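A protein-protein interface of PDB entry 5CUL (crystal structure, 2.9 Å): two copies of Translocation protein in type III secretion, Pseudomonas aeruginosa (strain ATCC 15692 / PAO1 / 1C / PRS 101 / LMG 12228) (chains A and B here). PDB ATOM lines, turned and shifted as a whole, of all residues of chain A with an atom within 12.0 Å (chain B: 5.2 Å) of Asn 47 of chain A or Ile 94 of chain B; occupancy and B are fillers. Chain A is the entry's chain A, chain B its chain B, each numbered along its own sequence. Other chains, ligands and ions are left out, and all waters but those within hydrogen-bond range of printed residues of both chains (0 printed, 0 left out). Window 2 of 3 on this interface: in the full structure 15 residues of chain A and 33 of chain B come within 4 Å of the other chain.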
ATOM      1  N   VAL A  43     -19.557   4.694  -7.896  1.00  0.00           N
ATOM      2  CA  VAL A  43     -19.533   5.368  -9.182  1.00  0.00           C
ATOM      3  C   VAL A  43     -19.282   6.848  -8.988  1.00  0.00           C
ATOM      4  O   VAL A  43     -19.695   7.424  -7.998  1.00  0.00           O
ATOM      5  CB  VAL A  43     -20.873   5.178  -9.935  1.00  0.00           C
ATOM      6  CG1 VAL A  43     -22.065   5.684  -9.103  1.00  0.00           C
ATOM      7  CG2 VAL A  43     -20.834   5.861 -11.307  1.00  0.00           C
ATOM      8  N   ILE A  44     -18.587   7.453  -9.934  1.00  0.00           N
ATOM      9  CA  ILE A  44     -18.341   8.892  -9.900  1.00  0.00           C
ATOM     10  C   ILE A  44     -19.204   9.503 -10.982  1.00  0.00           C
ATOM     11  O   ILE A  44     -19.173   9.094 -12.131  1.00  0.00           O
ATOM     12  CB  ILE A  44     -16.845   9.260 -10.143  1.00  0.00           C
ATOM     13  CG1 ILE A  44     -15.906   8.571  -9.123  1.00  0.00           C
ATOM     14  CG2 ILE A  44     -16.648  10.766 -10.118  1.00  0.00           C
ATOM     15  CD1 ILE A  44     -15.957   9.134  -7.734  1.00  0.00           C
ATOM     16  N   VAL A  45     -19.986  10.485 -10.609  1.00  0.00           N
ATOM     17  CA  VAL A  45     -20.755  11.202 -11.578  1.00  0.00           C
ATOM     18  C   VAL A  45     -19.999  12.467 -11.940  1.00  0.00           C
ATOM     19  O   VAL A  45     -19.717  13.278 -11.106  1.00  0.00           O
ATOM     20  CB  VAL A  45     -22.135  11.580 -11.028  1.00  0.00           C
ATOM     21  CG1 VAL A  45     -22.980  12.231 -12.114  1.00  0.00           C
ATOM     22  CG2 VAL A  45     -22.851  10.353 -10.505  1.00  0.00           C
ATOM     23  N   ALA A  46     -19.717  12.634 -13.214  1.00  0.00           N
ATOM     24  CA  ALA A  46     -19.015  13.781 -13.684  1.00  0.00           C
ATOM     25  C   ALA A  46     -19.866  14.549 -14.696  1.00  0.00           C
ATOM     26  O   ALA A  46     -20.874  14.064 -15.155  1.00  0.00           O
ATOM     27  CB  ALA A  46     -17.680  13.329 -14.305  1.00  0.00           C
ATOM     28  N   ASN A  47     -19.428  15.757 -15.021  1.00  0.00           N
ATOM     29  CA  ASN A  47     -20.018  16.559 -16.086  1.00  0.00           C
ATOM     30  C   ASN A  47     -19.189  16.460 -17.374  1.00  0.00           C
ATOM     31  O   ASN A  47     -18.204  15.713 -17.434  1.00  0.00           O
ATOM     32  CB  ASN A  47     -20.147  18.026 -15.668  1.00  0.00           C
ATOM     33  CG  ASN A  47     -18.814  18.686 -15.462  1.00  0.00           C
ATOM     34  OD1 ASN A  47     -17.762  18.040 -15.565  1.00  0.00           O
ATOM     35  ND2 ASN A  47     -18.843  19.975 -15.156  1.00  0.00           N
ATOM     36  N   PRO B  48     -18.286  26.378 -13.327  1.00  0.00           N
ATOM     37  CA  PRO B  48     -18.125  25.129 -12.552  1.00  0.00           C
ATOM     38  C   PRO B  48     -17.345  24.077 -13.359  1.00  0.00           C
ATOM     39  O   PRO B  48     -17.612  22.881 -13.262  1.00  0.00           O
ATOM     40  CB  PRO B  48     -19.593  24.709 -12.309  1.00  0.00           C
ATOM     41  CG  PRO B  48     -20.308  25.172 -13.572  1.00  0.00           C
ATOM     42  CD  PRO B  48     -19.610  26.463 -13.988  1.00  0.00           C
ATOM     43  N   THR B  49     -16.364  24.550 -14.122  1.00  0.00           N
ATOM     44  CA  THR B  49     -15.804  23.840 -15.274  1.00  0.00           C
ATOM     45  C   THR B  49     -15.814  22.329 -15.131  1.00  0.00           C
ATOM     46  O   THR B  49     -16.295  21.638 -16.032  1.00  0.00           O
ATOM     47  CB  THR B  49     -14.359  24.303 -15.551  1.00  0.00           C
ATOM     48  OG1 THR B  49     -14.352  25.732 -15.706  1.00  0.00           O
ATOM     49  CG2 THR B  49     -13.762  23.617 -16.830  1.00  0.00           C
ATOM     50  N   HIS B  50     -15.273  21.829 -14.018  1.00  0.00           N
ATOM     51  CA  HIS B  50     -15.242  20.383 -13.761  1.00  0.00           C
ATOM     52  C   HIS B  50     -16.001  20.024 -12.498  1.00  0.00           C
ATOM     53  O   HIS B  50     -16.026  20.778 -11.552  1.00  0.00           O
ATOM     54  CB  HIS B  50     -13.814  19.849 -13.688  1.00  0.00           C
ATOM     55  CG  HIS B  50     -13.101  19.850 -15.005  1.00  0.00           C
ATOM     56  ND1 HIS B  50     -13.415  18.975 -16.023  1.00  0.00           N
ATOM     57  CD2 HIS B  50     -12.091  20.621 -15.472  1.00  0.00           C
ATOM     58  CE1 HIS B  50     -12.622  19.199 -17.058  1.00  0.00           C
ATOM     59  NE2 HIS B  50     -11.812  20.198 -16.750  1.00  0.00           N
ATOM     60  N   VAL B  51     -16.650  18.869 -12.521  1.00  0.00           N
ATOM     61  CA  VAL B  51     -17.496  18.430 -11.430  1.00  0.00           C
ATOM     62  C   VAL B  51     -17.284  16.933 -11.295  1.00  0.00           C
ATOM     63  O   VAL B  51     -17.201  16.219 -12.293  1.00  0.00           O
ATOM     64  CB  VAL B  51     -19.008  18.749 -11.658  1.00  0.00           C
ATOM     65  CG1 VAL B  51     -19.911  17.910 -10.768  1.00  0.00           C
ATOM     66  CG2 VAL B  51     -19.320  20.221 -11.409  1.00  0.00           C
ATOM     67  N   ARG B  80     -11.070  11.886 -10.679  1.00  0.00           N
ATOM     68  CA  ARG B  80     -11.246  11.042 -11.865  1.00  0.00           C
ATOM     69  C   ARG B  80     -10.042  10.202 -12.151  1.00  0.00           C
ATOM     70  O   ARG B  80     -10.168   9.059 -12.545  1.00  0.00           O
ATOM     71  CB  ARG B  80     -11.588  11.878 -13.096  1.00  0.00           C
ATOM     72  CG  ARG B  80     -13.064  12.289 -13.132  1.00  0.00           C
ATOM     73  CD  ARG B  80     -13.297  13.592 -13.896  1.00  0.00           C
ATOM     74  NE  ARG B  80     -13.327  13.419 -15.357  1.00  0.00           N
ATOM     75  CZ  ARG B  80     -13.819  14.321 -16.213  1.00  0.00           C
ATOM     76  NH1 ARG B  80     -14.340  15.477 -15.771  1.00  0.00           N
ATOM     77  NH2 ARG B  80     -13.803  14.067 -17.521  1.00  0.00           N
ATOM     78  N   GLN B  92     -20.373  10.245 -17.118  1.00  0.00           N
ATOM     79  CA  GLN B  92     -20.760  11.614 -17.396  1.00  0.00           C
ATOM     80  C   GLN B  92     -22.279  11.789 -17.431  1.00  0.00           C
ATOM     81  O   GLN B  92     -22.951  11.330 -18.328  1.00  0.00           O
ATOM     82  CB  GLN B  92     -20.168  12.074 -18.719  1.00  0.00           C
ATOM     83  CG  GLN B  92     -20.335  13.574 -18.966  1.00  0.00           C
ATOM     84  CD  GLN B  92     -19.637  14.052 -20.232  1.00  0.00           C
ATOM     85  OE1 GLN B  92     -18.667  14.834 -20.167  1.00  0.00           O
ATOM     86  NE2 GLN B  92     -20.117  13.574 -21.399  1.00  0.00           N
ATOM     87  N   ARG B  93     -22.804  12.466 -16.431  1.00  0.00           N
ATOM     88  CA  ARG B  93     -24.193  12.814 -16.375  1.00  0.00           C
ATOM     89  C   ARG B  93     -24.264  14.262 -15.961  1.00  0.00           C
ATOM     90  O   ARG B  93     -24.260  14.568 -14.787  1.00  0.00           O
ATOM     91  CB  ARG B  93     -24.913  11.935 -15.372  1.00  0.00           C
ATOM     92  CG  ARG B  93     -24.942  10.465 -15.737  1.00  0.00           C
ATOM     93  CD  ARG B  93     -25.771  10.205 -16.990  1.00  0.00           C
ATOM     94  NE  ARG B  93     -26.078   8.784 -17.179  1.00  0.00           N
ATOM     95  CZ  ARG B  93     -25.429   7.942 -17.997  1.00  0.00           C
ATOM     96  NH1 ARG B  93     -24.404   8.343 -18.727  1.00  0.00           N
ATOM     97  NH2 ARG B  93     -25.815   6.671 -18.086  1.00  0.00           N
ATOM     98  N   ILE B  94     -24.325  15.144 -16.952  1.00  0.00           N
ATOM     99  CA  ILE B  94     -24.158  16.592 -16.738  1.00  0.00           C
ATOM    100  C   ILE B  94     -25.278  17.286 -15.966  1.00  0.00           C
ATOM    101  O   ILE B  94     -24.991  18.091 -15.060  1.00  0.00           O
ATOM    102  CB  ILE B  94     -23.933  17.334 -18.080  1.00  0.00           C
ATOM    103  CG1 ILE B  94     -22.721  16.726 -18.818  1.00  0.00           C
ATOM    104  CG2 ILE B  94     -23.757  18.829 -17.842  1.00  0.00           C
ATOM    105  CD1 ILE B  94     -22.196  17.528 -19.987  1.00  0.00           C
ATOM    106  N   PRO B  95     -26.552  17.013 -16.332  1.00  0.00           N
ATOM    107  CA  PRO B  95     -27.604  17.676 -15.534  1.00  0.00           C
ATOM    108  C   PRO B  95     -27.650  17.155 -14.094  1.00  0.00           C
ATOM    109  O   PRO B  95     -27.929  17.927 -13.179  1.00  0.00           O
ATOM    110  CB  PRO B  95     -28.905  17.335 -16.277  1.00  0.00           C
ATOM    111  CG  PRO B  95     -28.477  16.874 -17.635  1.00  0.00           C
ATOM    112  CD  PRO B  95     -27.125  16.229 -17.442  1.00  0.00           C
ATOM    113  N   LEU B  96     -27.383  15.858 -13.916  1.00  0.00           N
ATOM    114  CA  LEU B  96     -27.333  15.239 -12.584  1.00  0.00           C
ATOM    115  C   LEU B  96     -26.143  15.731 -11.768  1.00  0.00           C
ATOM    116  O   LEU B  96     -26.288  16.050 -10.602  1.00  0.00           O
ATOM    117  CB  LEU B  96     -27.247  13.718 -12.687  1.00  0.00           C
ATOM    118  CG  LEU B  96     -27.171  12.976 -11.359  1.00  0.00           C
ATOM    119  CD1 LEU B  96     -28.367  13.336 -10.487  1.00  0.00           C
ATOM    120  CD2 LEU B  96     -27.133  11.486 -11.603  1.00  0.00           C
ATOM    121  N   ALA B  97     -24.966  15.770 -12.384  1.00  0.00           N
ATOM    122  CA  ALA B  97     -23.754  16.271 -11.729  1.00  0.00           C
ATOM    123  C   ALA B  97     -23.973  17.701 -11.238  1.00  0.00           C
ATOM    124  O   ALA B  97     -23.700  17.994 -10.075  1.00  0.00           O
ATOM    125  CB  ALA B  97     -22.562  16.212 -12.678  1.00  0.00           C
ATOM    126  N   ARG B  98     -24.491  18.580 -12.100  1.00  0.00           N
ATOM    127  CA  ARG B  98     -24.807  19.953 -11.685  1.00  0.00           C
ATOM    128  C   ARG B  98     -25.801  19.991 -10.504  1.00  0.00           C
ATOM    129  O   ARG B  98     -25.618  20.698  -9.527  1.00  0.00           O
ATOM    130  CB  ARG B  98     -25.399  20.724 -12.855  1.00  0.00           C
ATOM    131  CG  ARG B  98     -24.367  21.379 -13.747  1.00  0.00           C
ATOM    132  CD  ARG B  98     -24.978  22.587 -14.456  1.00  0.00           C
ATOM    133  NE  ARG B  98     -25.940  22.214 -15.505  1.00  0.00           N
ATOM    134  CZ  ARG B  98     -25.623  22.019 -16.790  1.00  0.00           C
ATOM    135  NH1 ARG B  98     -24.355  22.134 -17.215  1.00  0.00           N
ATOM    136  NH2 ARG B  98     -26.578  21.700 -17.669  1.00  0.00           N
ATOM    137  N   ALA B  99     -26.868  19.229 -10.618  1.00  0.00           N
ATOM    138  CA  ALA B  99     -27.870  19.171  -9.574  1.00  0.00           C
ATOM    139  C   ALA B  99     -27.282  18.638  -8.290  1.00  0.00           C
ATOM    140  O   ALA B  99     -27.486  19.217  -7.238  1.00  0.00           O
ATOM    141  CB  ALA B  99     -29.033  18.296 -10.026  1.00  0.00           C
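Of the 13 printed residues of chain B, 8 touch a printed residue of chain A. Among the printed residues, 12 pairs touch across the chains.
The backbone carbonyl oxygen of Ala 46 of chain A is in hydrogen-bond range of the backbone NH of Arg 93 of chain B (2.8 Å). ND2 of Asn 47 of chain A sits at hydrogen-bond distance from O of Thr 49 of chain B. The side-chain amide oxygen (OD1) of Asn 47 of chain A is in hydrogen-bond range of the backbone NH (N) of Val 51 of chain B. The backbone carbonyl oxygen of Asn 47 of chain A lies close to the side-chain amide oxygen of Gln 92 of chain B, 2.9 Å away.
Arg 93 of chain B touches Val 45 of chain A (O to CG1, 3.8 Å). CA of Ala 46 of chain A touches O of Val 51 of chain B, at 3.3 Å. Ala 46 of chain A touches Gln 92 of chain B (O to CA, 3.3 Å). Ala 97 of chain B touches Ala 46 of chain A (CB to O, 3.7 Å). Pro 48 of chain B touches Asn 47 of chain A. CA of His 50 of chain B touches ND2 of Asn 47 of chain A, at 3.9 Å. Asn 47 of chain A touches Ile 94 of chain B. Asn 47 of chain A touches Ala 97 of chain B (N to CB, 3.9 Å).
Asn 47 of chain A touches just these residues of chain B: Pro 48, Thr 49, His 50, Val 51, Gln 92, Ile 94 and Ala 97. Ile 94 of chain B touches one residue of chain A. Pro 48 of chain B touches one residue of chain A. Of chain A, only Asn 47 (3.2 Å) comes within 4 Å of Thr 49 of chain B. Of chain A, only Ala 46 and Asn 47 come within 4 Å of Ala 97 of chain B. No residue of chain A comes within 4 Å of Arg 98 of chain B. Printed residues of chain B within 4 Å of Val 45 of chain A: Arg 93 (3.8 Å). Of the printed residues of chain B, Ala 46 of chain A touches Val 51 (3.3 Å), Gln 92 (3.3 Å), Arg 93 (2.8 Å) and Ala 97 (3.7 Å). Of the printed residues of chain A, Arg 93 of chain B touches Val 45 and Ala 46. Val 43 of chain A touches none of the printed residues of chain B. The nearest residue of chain B that does not touch Asn 47 of chain A is Arg 80 of chain B (4.2 Å). The nearest printed residue of chain B that does not touch Val 45 of chain A is Ala 97 of chain B (4.04 Å).
No position is printed for both chains. Of the 12 pairs that touch across the chains among the printed residues, none has its exchanged pair printed and touching as well.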
